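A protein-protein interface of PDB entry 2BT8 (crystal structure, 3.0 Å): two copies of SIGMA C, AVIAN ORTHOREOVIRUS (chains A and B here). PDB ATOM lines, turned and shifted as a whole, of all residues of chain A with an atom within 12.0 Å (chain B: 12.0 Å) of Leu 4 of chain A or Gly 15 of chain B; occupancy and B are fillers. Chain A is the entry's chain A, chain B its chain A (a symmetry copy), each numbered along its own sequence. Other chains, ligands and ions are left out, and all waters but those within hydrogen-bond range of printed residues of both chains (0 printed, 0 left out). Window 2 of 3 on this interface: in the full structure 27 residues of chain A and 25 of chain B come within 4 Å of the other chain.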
ATOM      1  N   SER A   1     -37.007  -8.927 -28.204  1.00  0.00           N
ATOM      2  CA  SER A   1     -38.280  -9.483 -28.758  1.00  0.00           C
ATOM      3  C   SER A   1     -38.172 -10.992 -28.996  1.00  0.00           C
ATOM      4  O   SER A   1     -39.169 -11.714 -28.894  1.00  0.00           O
ATOM      5  CB  SER A   1     -38.641  -8.786 -30.089  1.00  0.00           C
ATOM      6  OG  SER A   1     -37.903  -7.585 -30.308  1.00  0.00           O
ATOM      7  N   HIS A   2     -36.933 -11.434 -29.267  1.00  0.00           N
ATOM      8  CA  HIS A   2     -36.618 -12.643 -30.062  1.00  0.00           C
ATOM      9  C   HIS A   2     -35.627 -13.631 -29.441  1.00  0.00           C
ATOM     10  O   HIS A   2     -35.516 -14.742 -29.943  1.00  0.00           O
ATOM     11  CB  HIS A   2     -36.100 -12.266 -31.477  1.00  0.00           C
ATOM     12  CG  HIS A   2     -37.060 -11.450 -32.301  1.00  0.00           C
ATOM     13  ND1 HIS A   2     -36.779 -10.160 -32.711  1.00  0.00           N
ATOM     14  CD2 HIS A   2     -38.288 -11.744 -32.798  1.00  0.00           C
ATOM     15  CE1 HIS A   2     -37.796  -9.693 -33.415  1.00  0.00           C
ATOM     16  NE2 HIS A   2     -38.723 -10.634 -33.483  1.00  0.00           N
ATOM     17  N   GLY A   3     -34.863 -13.216 -28.431  1.00  0.00           N
ATOM     18  CA  GLY A   3     -34.211 -14.157 -27.476  1.00  0.00           C
ATOM     19  C   GLY A   3     -33.004 -15.030 -27.841  1.00  0.00           C
ATOM     20  O   GLY A   3     -31.976 -14.526 -28.321  1.00  0.00           O
ATOM     21  N   LEU A   4     -33.096 -16.337 -27.569  1.00  0.00           N
ATOM     22  CA  LEU A   4     -32.103 -17.278 -28.115  1.00  0.00           C
ATOM     23  C   LEU A   4     -32.606 -18.693 -28.474  1.00  0.00           C
ATOM     24  O   LEU A   4     -33.357 -19.324 -27.717  1.00  0.00           O
ATOM     25  CB  LEU A   4     -30.781 -17.248 -27.317  1.00  0.00           C
ATOM     26  CG  LEU A   4     -30.209 -18.340 -26.416  1.00  0.00           C
ATOM     27  CD1 LEU A   4     -29.128 -17.808 -25.469  1.00  0.00           C
ATOM     28  CD2 LEU A   4     -31.286 -19.005 -25.614  1.00  0.00           C
ATOM     29  N   SER A   5     -32.187 -19.167 -29.651  1.00  0.00           N
ATOM     30  CA  SER A   5     -32.544 -20.515 -30.176  1.00  0.00           C
ATOM     31  C   SER A   5     -31.374 -21.512 -30.344  1.00  0.00           C
ATOM     32  O   SER A   5     -30.194 -21.138 -30.207  1.00  0.00           O
ATOM     33  CB  SER A   5     -33.289 -20.378 -31.505  1.00  0.00           C
ATOM     34  OG  SER A   5     -34.681 -20.495 -31.305  1.00  0.00           O
ATOM     35  N   PHE A   6     -31.720 -22.771 -30.654  1.00  0.00           N
ATOM     36  CA  PHE A   6     -30.730 -23.871 -30.883  1.00  0.00           C
ATOM     37  C   PHE A   6     -30.937 -24.689 -32.185  1.00  0.00           C
ATOM     38  O   PHE A   6     -32.000 -25.302 -32.393  1.00  0.00           O
ATOM     39  CB  PHE A   6     -30.709 -24.806 -29.679  1.00  0.00           C
ATOM     40  CG  PHE A   6     -30.455 -24.102 -28.376  1.00  0.00           C
ATOM     41  CD1 PHE A   6     -29.155 -23.853 -27.941  1.00  0.00           C
ATOM     42  CD2 PHE A   6     -31.511 -23.676 -27.580  1.00  0.00           C
ATOM     43  CE1 PHE A   6     -28.909 -23.193 -26.729  1.00  0.00           C
ATOM     44  CE2 PHE A   6     -31.271 -23.016 -26.368  1.00  0.00           C
ATOM     45  CZ  PHE A   6     -29.967 -22.781 -25.942  1.00  0.00           C
ATOM     46  N   SER A   7     -29.925 -24.705 -33.060  1.00  0.00           N
ATOM     47  CA  SER A   7     -29.997 -25.491 -34.323  1.00  0.00           C
ATOM     48  C   SER A   7     -29.426 -26.904 -34.177  1.00  0.00           C
ATOM     49  O   SER A   7     -28.528 -27.138 -33.355  1.00  0.00           O
ATOM     50  CB  SER A   7     -29.324 -24.767 -35.487  1.00  0.00           C
ATOM     51  OG  SER A   7     -28.083 -24.263 -35.061  1.00  0.00           O
ATOM     52  N   PRO A   8     -29.961 -27.854 -34.967  1.00  0.00           N
ATOM     53  CA  PRO A   8     -29.522 -29.256 -34.871  1.00  0.00           C
ATOM     54  C   PRO A   8     -28.008 -29.369 -35.101  1.00  0.00           C
ATOM     55  O   PRO A   8     -27.469 -28.597 -35.886  1.00  0.00           O
ATOM     56  CB  PRO A   8     -30.326 -29.950 -35.975  1.00  0.00           C
ATOM     57  CG  PRO A   8     -31.550 -29.062 -36.161  1.00  0.00           C
ATOM     58  CD  PRO A   8     -31.011 -27.678 -35.988  1.00  0.00           C
ATOM     59  N   LEU A  10     -28.298 -29.785 -31.915  1.00  0.00           N
ATOM     60  CA  LEU A  10     -28.785 -29.267 -30.631  1.00  0.00           C
ATOM     61  C   LEU A  10     -30.286 -29.154 -30.731  1.00  0.00           C
ATOM     62  O   LEU A  10     -30.812 -28.746 -31.771  1.00  0.00           O
ATOM     63  CB  LEU A  10     -28.180 -27.905 -30.329  1.00  0.00           C
ATOM     64  CG  LEU A  10     -26.692 -27.908 -30.029  1.00  0.00           C
ATOM     65  CD1 LEU A  10     -26.149 -26.500 -30.011  1.00  0.00           C
ATOM     66  CD2 LEU A  10     -26.429 -28.591 -28.705  1.00  0.00           C
ATOM     67  N   SER A  11     -30.978 -29.560 -29.673  1.00  0.00           N
ATOM     68  CA  SER A  11     -32.431 -29.398 -29.621  1.00  0.00           C
ATOM     69  C   SER A  11     -32.937 -29.145 -28.183  1.00  0.00           C
ATOM     70  O   SER A  11     -32.186 -29.285 -27.199  1.00  0.00           O
ATOM     71  CB  SER A  11     -33.153 -30.589 -30.271  1.00  0.00           C
ATOM     72  OG  SER A  11     -33.459 -31.570 -29.293  1.00  0.00           O
ATOM     73  N   VAL A  12     -34.206 -28.762 -28.062  1.00  0.00           N
ATOM     74  CA  VAL A  12     -34.748 -28.444 -26.744  1.00  0.00           C
ATOM     75  C   VAL A  12     -36.152 -28.999 -26.484  1.00  0.00           C
ATOM     76  O   VAL A  12     -36.977 -29.071 -27.378  1.00  0.00           O
ATOM     77  CB  VAL A  12     -34.582 -26.930 -26.425  1.00  0.00           C
ATOM     78  CG1 VAL A  12     -34.755 -26.098 -27.684  1.00  0.00           C
ATOM     79  CG2 VAL A  12     -35.492 -26.480 -25.297  1.00  0.00           C
ATOM     80  N   ALA A  13     -36.388 -29.454 -25.262  1.00  0.00           N
ATOM     81  CA  ALA A  13     -37.688 -29.970 -24.905  1.00  0.00           C
ATOM     82  C   ALA A  13     -37.933 -29.695 -23.432  1.00  0.00           C
ATOM     83  O   ALA A  13     -37.157 -30.165 -22.569  1.00  0.00           O
ATOM     84  CB  ALA A  13     -37.796 -31.445 -25.220  1.00  0.00           C
ATOM     85  N   ASP A  14     -39.006 -28.917 -23.169  1.00  0.00           N
ATOM     86  CA  ASP A  14     -39.361 -28.411 -21.830  1.00  0.00           C
ATOM     87  C   ASP A  14     -38.215 -27.617 -21.279  1.00  0.00           C
ATOM     88  O   ASP A  14     -37.797 -27.855 -20.149  1.00  0.00           O
ATOM     89  CB  ASP A  14     -39.656 -29.547 -20.847  1.00  0.00           C
ATOM     90  CG  ASP A  14     -40.717 -30.497 -21.357  1.00  0.00           C
ATOM     91  OD1 ASP A  14     -40.730 -30.824 -22.579  1.00  0.00           O
ATOM     92  OD2 ASP A  14     -41.539 -30.928 -20.515  1.00  0.00           O
ATOM     93  N   GLY A  15     -37.684 -26.711 -22.090  1.00  0.00           N
ATOM     94  CA  GLY A  15     -36.516 -25.928 -21.705  1.00  0.00           C
ATOM     95  C   GLY A  15     -35.361 -26.741 -21.138  1.00  0.00           C
ATOM     96  O   GLY A  15     -34.739 -26.349 -20.127  1.00  0.00           O
ATOM     97  N   VAL A  16     -35.106 -27.894 -21.762  1.00  0.00           N
ATOM     98  CA  VAL A  16     -33.908 -28.691 -21.491  1.00  0.00           C
ATOM     99  C   VAL A  16     -33.216 -28.820 -22.818  1.00  0.00           C
ATOM    100  O   VAL A  16     -33.787 -29.375 -23.747  1.00  0.00           O
ATOM    101  CB  VAL A  16     -34.225 -30.102 -20.959  1.00  0.00           C
ATOM    102  CG1 VAL A  16     -32.955 -30.771 -20.503  1.00  0.00           C
ATOM    103  CG2 VAL A  16     -35.218 -30.047 -19.811  1.00  0.00           C
ATOM    104  N   VAL A  17     -32.006 -28.280 -22.919  1.00  0.00           N
ATOM    105  CA  VAL A  17     -31.231 -28.344 -24.167  1.00  0.00           C
ATOM    106  C   VAL A  17     -30.346 -29.597 -24.226  1.00  0.00           C
ATOM    107  O   VAL A  17     -29.676 -29.967 -23.251  1.00  0.00           O
ATOM    108  CB  VAL A  17     -30.400 -27.061 -24.392  1.00  0.00           C
ATOM    109  CG1 VAL A  17     -29.580 -27.143 -25.675  1.00  0.00           C
ATOM    110  CG2 VAL A  17     -31.311 -25.851 -24.437  1.00  0.00           C
ATOM    111  N   SER A  18     -30.366 -30.239 -25.387  1.00  0.00           N
ATOM    112  CA  SER A  18     -29.727 -31.526 -25.590  1.00  0.00           C
ATOM    113  C   SER A  18     -28.857 -31.630 -26.825  1.00  0.00           C
ATOM    114  O   SER A  18     -29.061 -30.924 -27.837  1.00  0.00           O
ATOM    115  CB  SER A  18     -30.797 -32.586 -25.713  1.00  0.00           C
ATOM    116  OG  SER A  18     -30.926 -33.223 -24.478  1.00  0.00           O
ATOM    117  N   HIS B   2     -24.696 -10.487 -15.960  1.00  0.00           N
ATOM    118  CA  HIS B   2     -23.697 -11.213 -16.778  1.00  0.00           C
ATOM    119  C   HIS B   2     -24.193 -12.465 -17.509  1.00  0.00           C
ATOM    120  O   HIS B   2     -23.479 -12.959 -18.371  1.00  0.00           O
ATOM    121  CB  HIS B   2     -22.457 -11.608 -15.931  1.00  0.00           C
ATOM    122  CG  HIS B   2     -21.732 -10.450 -15.300  1.00  0.00           C
ATOM    123  ND1 HIS B   2     -21.638 -10.287 -13.931  1.00  0.00           N
ATOM    124  CD2 HIS B   2     -21.059  -9.408 -15.849  1.00  0.00           C
ATOM    125  CE1 HIS B   2     -20.948  -9.191 -13.666  1.00  0.00           C
ATOM    126  NE2 HIS B   2     -20.586  -8.640 -14.813  1.00  0.00           N
ATOM    127  N   GLY B   3     -25.341 -13.016 -17.118  1.00  0.00           N
ATOM    128  CA  GLY B   3     -26.135 -13.924 -17.995  1.00  0.00           C
ATOM    129  C   GLY B   3     -25.719 -15.365 -18.317  1.00  0.00           C
ATOM    130  O   GLY B   3     -25.467 -16.173 -17.409  1.00  0.00           O
ATOM    131  N   LEU B   4     -25.694 -15.715 -19.608  1.00  0.00           N
ATOM    132  CA  LEU B   4     -25.066 -16.982 -20.020  1.00  0.00           C
ATOM    133  C   LEU B   4     -24.363 -16.998 -21.394  1.00  0.00           C
ATOM    134  O   LEU B   4     -24.887 -16.487 -22.394  1.00  0.00           O
ATOM    135  CB  LEU B   4     -25.985 -18.194 -19.753  1.00  0.00           C
ATOM    136  CG  LEU B   4     -26.685 -19.080 -20.779  1.00  0.00           C
ATOM    137  CD1 LEU B   4     -27.831 -19.892 -20.165  1.00  0.00           C
ATOM    138  CD2 LEU B   4     -27.212 -18.272 -21.927  1.00  0.00           C
ATOM    139  N   SER B   5     -23.161 -17.583 -21.415  1.00  0.00           N
ATOM    140  CA  SER B   5     -22.326 -17.717 -22.642  1.00  0.00           C
ATOM    141  C   SER B   5     -22.072 -19.161 -23.137  1.00  0.00           C
ATOM    142  O   SER B   5     -22.408 -20.140 -22.444  1.00  0.00           O
ATOM    143  CB  SER B   5     -20.989 -17.005 -22.444  1.00  0.00           C
ATOM    144  OG  SER B   5     -21.014 -15.731 -23.050  1.00  0.00           O
ATOM    145  N   PHE B   6     -21.466 -19.271 -24.328  1.00  0.00           N
ATOM    146  CA  PHE B   6     -21.111 -20.580 -24.962  1.00  0.00           C
ATOM    147  C   PHE B   6     -19.650 -20.696 -25.472  1.00  0.00           C
ATOM    148  O   PHE B   6     -19.208 -19.910 -26.329  1.00  0.00           O
ATOM    149  CB  PHE B   6     -22.083 -20.887 -26.096  1.00  0.00           C
ATOM    150  CG  PHE B   6     -23.525 -20.854 -25.675  1.00  0.00           C
ATOM    151  CD1 PHE B   6     -24.136 -21.981 -25.129  1.00  0.00           C
ATOM    152  CD2 PHE B   6     -24.280 -19.696 -25.816  1.00  0.00           C
ATOM    153  CE1 PHE B   6     -25.480 -21.957 -24.730  1.00  0.00           C
ATOM    154  CE2 PHE B   6     -25.624 -19.667 -25.419  1.00  0.00           C
ATOM    155  CZ  PHE B   6     -26.223 -20.802 -24.882  1.00  0.00           C
ATOM    156  N   SER B   7     -18.902 -21.676 -24.951  1.00  0.00           N
ATOM    157  CA  SER B   7     -17.500 -21.907 -25.397  1.00  0.00           C
ATOM    158  C   SER B   7     -17.398 -22.920 -26.540  1.00  0.00           C
ATOM    159  O   SER B   7     -18.240 -23.823 -26.658  1.00  0.00           O
ATOM    160  CB  SER B   7     -16.593 -22.324 -24.241  1.00  0.00           C
ATOM    161  OG  SER B   7     -17.243 -23.309 -23.477  1.00  0.00           O
ATOM    162  N   LEU B  10     -19.097 -24.900 -29.348  1.00  0.00           N
ATOM    163  CA  LEU B  10     -20.405 -24.234 -29.335  1.00  0.00           C
ATOM    164  C   LEU B  10     -20.177 -22.786 -29.694  1.00  0.00           C
ATOM    165  O   LEU B  10     -19.199 -22.180 -29.245  1.00  0.00           O
ATOM    166  CB  LEU B  10     -21.052 -24.333 -27.961  1.00  0.00           C
ATOM    167  CG  LEU B  10     -21.497 -25.726 -27.553  1.00  0.00           C
ATOM    168  CD1 LEU B  10     -21.871 -25.758 -26.091  1.00  0.00           C
ATOM    169  CD2 LEU B  10     -22.663 -26.170 -28.405  1.00  0.00           C
ATOM    170  N   SER B  11     -21.046 -22.247 -30.539  1.00  0.00           N
ATOM    171  CA  SER B  11     -20.981 -20.824 -30.874  1.00  0.00           C
ATOM    172  C   SER B  11     -22.380 -20.226 -31.146  1.00  0.00           C
ATOM    173  O   SER B  11     -23.384 -20.955 -31.262  1.00  0.00           O
ATOM    174  CB  SER B  11     -20.021 -20.566 -32.046  1.00  0.00           C
ATOM    175  OG  SER B  11     -20.730 -20.586 -33.274  1.00  0.00           O
ATOM    176  N   VAL B  12     -22.447 -18.899 -31.235  1.00  0.00           N
ATOM    177  CA  VAL B  12     -23.740 -18.249 -31.430  1.00  0.00           C
ATOM    178  C   VAL B  12     -23.729 -17.110 -32.455  1.00  0.00           C
ATOM    179  O   VAL B  12     -22.760 -16.382 -32.577  1.00  0.00           O
ATOM    180  CB  VAL B  12     -24.390 -17.883 -30.065  1.00  0.00           C
ATOM    181  CG1 VAL B  12     -23.327 -17.470 -29.061  1.00  0.00           C
ATOM    182  CG2 VAL B  12     -25.488 -16.846 -30.213  1.00  0.00           C
ATOM    183  N   ALA B  13     -24.794 -17.011 -33.236  1.00  0.00           N
ATOM    184  CA  ALA B  13     -24.896 -15.955 -34.215  1.00  0.00           C
ATOM    185  C   ALA B  13     -26.361 -15.593 -34.390  1.00  0.00           C
ATOM    186  O   ALA B  13     -27.180 -16.461 -34.772  1.00  0.00           O
ATOM    187  CB  ALA B  13     -24.265 -16.362 -35.527  1.00  0.00           C
ATOM    188  N   ASP B  14     -26.672 -14.314 -34.087  1.00  0.00           N
ATOM    189  CA  ASP B  14     -28.044 -13.774 -34.054  1.00  0.00           C
ATOM    190  C   ASP B  14     -28.867 -14.568 -33.085  1.00  0.00           C
ATOM    191  O   ASP B  14     -29.958 -15.013 -33.435  1.00  0.00           O
ATOM    192  CB  ASP B  14     -28.725 -13.857 -35.423  1.00  0.00           C
ATOM    193  CG  ASP B  14     -27.917 -13.195 -36.516  1.00  0.00           C
ATOM    194  OD1 ASP B  14     -26.660 -13.324 -36.532  1.00  0.00           O
ATOM    195  OD2 ASP B  14     -28.559 -12.546 -37.377  1.00  0.00           O
ATOM    196  N   GLY B  15     -28.327 -14.781 -31.892  1.00  0.00           N
ATOM    197  CA  GLY B  15     -28.990 -15.603 -30.887  1.00  0.00           C
ATOM    198  C   GLY B  15     -29.486 -16.951 -31.390  1.00  0.00           C
ATOM    199  O   GLY B  15     -30.616 -17.377 -31.070  1.00  0.00           O
ATOM    200  N   VAL B  16     -28.660 -17.599 -32.217  1.00  0.00           N
ATOM    201  CA  VAL B  16     -28.877 -18.988 -32.623  1.00  0.00           C
ATOM    202  C   VAL B  16     -27.631 -19.717 -32.204  1.00  0.00           C
ATOM    203  O   VAL B  16     -26.552 -19.392 -32.679  1.00  0.00           O
ATOM    204  CB  VAL B  16     -29.059 -19.156 -34.144  1.00  0.00           C
ATOM    205  CG1 VAL B  16     -29.492 -20.565 -34.452  1.00  0.00           C
ATOM    206  CG2 VAL B  16     -30.084 -18.173 -34.687  1.00  0.00           C
ATOM    207  N   VAL B  17     -27.775 -20.674 -31.293  1.00  0.00           N
ATOM    208  CA  VAL B  17     -26.629 -21.456 -30.806  1.00  0.00           C
ATOM    209  C   VAL B  17     -26.395 -22.715 -31.653  1.00  0.00           C
ATOM    210  O   VAL B  17     -27.333 -23.445 -32.005  1.00  0.00           O
ATOM    211  CB  VAL B  17     -26.770 -21.808 -29.308  1.00  0.00           C
ATOM    212  CG1 VAL B  17     -25.591 -22.639 -28.815  1.00  0.00           C
ATOM    213  CG2 VAL B  17     -26.890 -20.541 -28.484  1.00  0.00           C
ATOM    214  N   SER B  18     -25.129 -22.944 -31.974  1.00  0.00           N
ATOM    215  CA  SER B  18     -24.722 -23.987 -32.898  1.00  0.00           C
ATOM    216  C   SER B  18     -23.590 -24.871 -32.420  1.00  0.00           C
ATOM    217  O   SER B  18     -22.737 -24.466 -31.601  1.00  0.00           O
ATOM    218  CB  SER B  18     -24.266 -23.343 -34.187  1.00  0.00           C
ATOM    219  OG  SER B  18     -25.316 -23.406 -35.104  1.00  0.00           O
ATOM    220  N   LEU B  19     -23.569 -26.081 -32.976  1.00  0.00           N
ATOM    221  CA  LEU B  19     -22.361 -26.909 -32.940  1.00  0.00           C
ATOM    222  C   LEU B  19     -21.507 -26.648 -34.176  1.00  0.00           C
ATOM    223  O   LEU B  19     -21.955 -26.876 -35.299  1.00  0.00           O
ATOM    224  CB  LEU B  19     -22.726 -28.381 -32.853  1.00  0.00           C
ATOM    225  CG  LEU B  19     -21.593 -29.270 -32.374  1.00  0.00           C
ATOM    226  CD1 LEU B  19     -20.739 -28.569 -31.323  1.00  0.00           C
ATOM    227  CD2 LEU B  19     -22.172 -30.558 -31.833  1.00  0.00           C
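The backbone carbonyl oxygen of Gly 15 of chain B sits at hydrogen-bond distance from the backbone NH of Ser 5 of chain A, at 2.8 Å. N of Ser 7 of chain A lies within hydrogen-bond range of O of Val 17 of chain B (3.1 Å). O of Ser 5 of chain A sits at hydrogen-bond distance from N of Val 17 of chain B (2.7 Å). OG of Ser 7 of chain A lies within hydrogen-bond range of OG of Ser 18 of chain B (2.9 Å).
The backbone NH of Ser 18 of chain B is in hydrogen-bond range of the backbone carbonyl oxygen of Ser 11 of chain B, 2.7 Å away.
Among the printed residues, pairs that only touch across the chains: Leu 4 of chain A with Phe 6 of chain B, Leu 4 of chain A with Gly 15 of chain B, Ser 5 of chain A with Val 16 of chain B, Phe 6 of chain A with Val 17 of chain B, Leu 10 of chain A with Leu 10 of chain B, Leu 10 of chain A with Val 17 of chain B, Leu 10 of chain A with Ser 18 of chain B and Leu 10 of chain A with Leu 19 of chain B.
Leu 4 of chain A touches two residues of chain B. Gly 15 of chain B touches two residues of chain A. No residue of chain B comes within 4 Å of Gly 3 of chain A. Of chain B, only Gly 15 (2.8 Å), Val 16 (3.5 Å) and Val 17 (2.7 Å) come within 4 Å of Ser 5 of chain A. Of chain B, only Val 17 (3.4 Å) comes within 4 Å of Phe 6 of chain A. Ala 13 of chain B touches none of the printed residues of chain A. No residue of chain A comes within 4 Å of Asp 14 of chain B. Val 17 of chain B touches just these residues of chain A: Ser 5 (2.7 Å), Phe 6 (3.4 Å), Ser 7 (3.1 Å) and Leu 10 (3.8 Å). Of the printed residues of chain A, Phe 6 of chain B touches Leu 4. Printed residues of chain B within 4 Å of Ser 7 of chain A: Val 17 and Ser 18. The nearest residue of chain A that does not touch Gly 15 of chain B is Gly 3 of chain A (4.1 Å).
Of the 16 printed residues of chain B, 7 touch a printed residue of chain A.
Leu 4 of chain A touches Gly 15 of chain B, but with the chains exchanged Gly 15 of chain A does not touch Leu 4 of chain B (9.5 Å). Ser 5 of chain A touches Val 16 of chain B, but with the chains exchanged Val 16 of chain A does not touch Ser 5 of chain B (13.9 Å). Ser 5 of chain A touches Val 17 of chain B, but with the chains exchanged Val 17 of chain A does not touch Ser 5 of chain B (10.5 Å). Leu 10 of chain B touches its own counterpart, Leu 10 of chain A. Positions printed for both chains: 2, 3, 4, 5, 6, 7, 10, 11, 12, 13, 14, 15, 16, 17 and 18. Of the 12 pairs that touch across the chains among the printed residues, 1 has its exchanged pair printed and touching as well.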
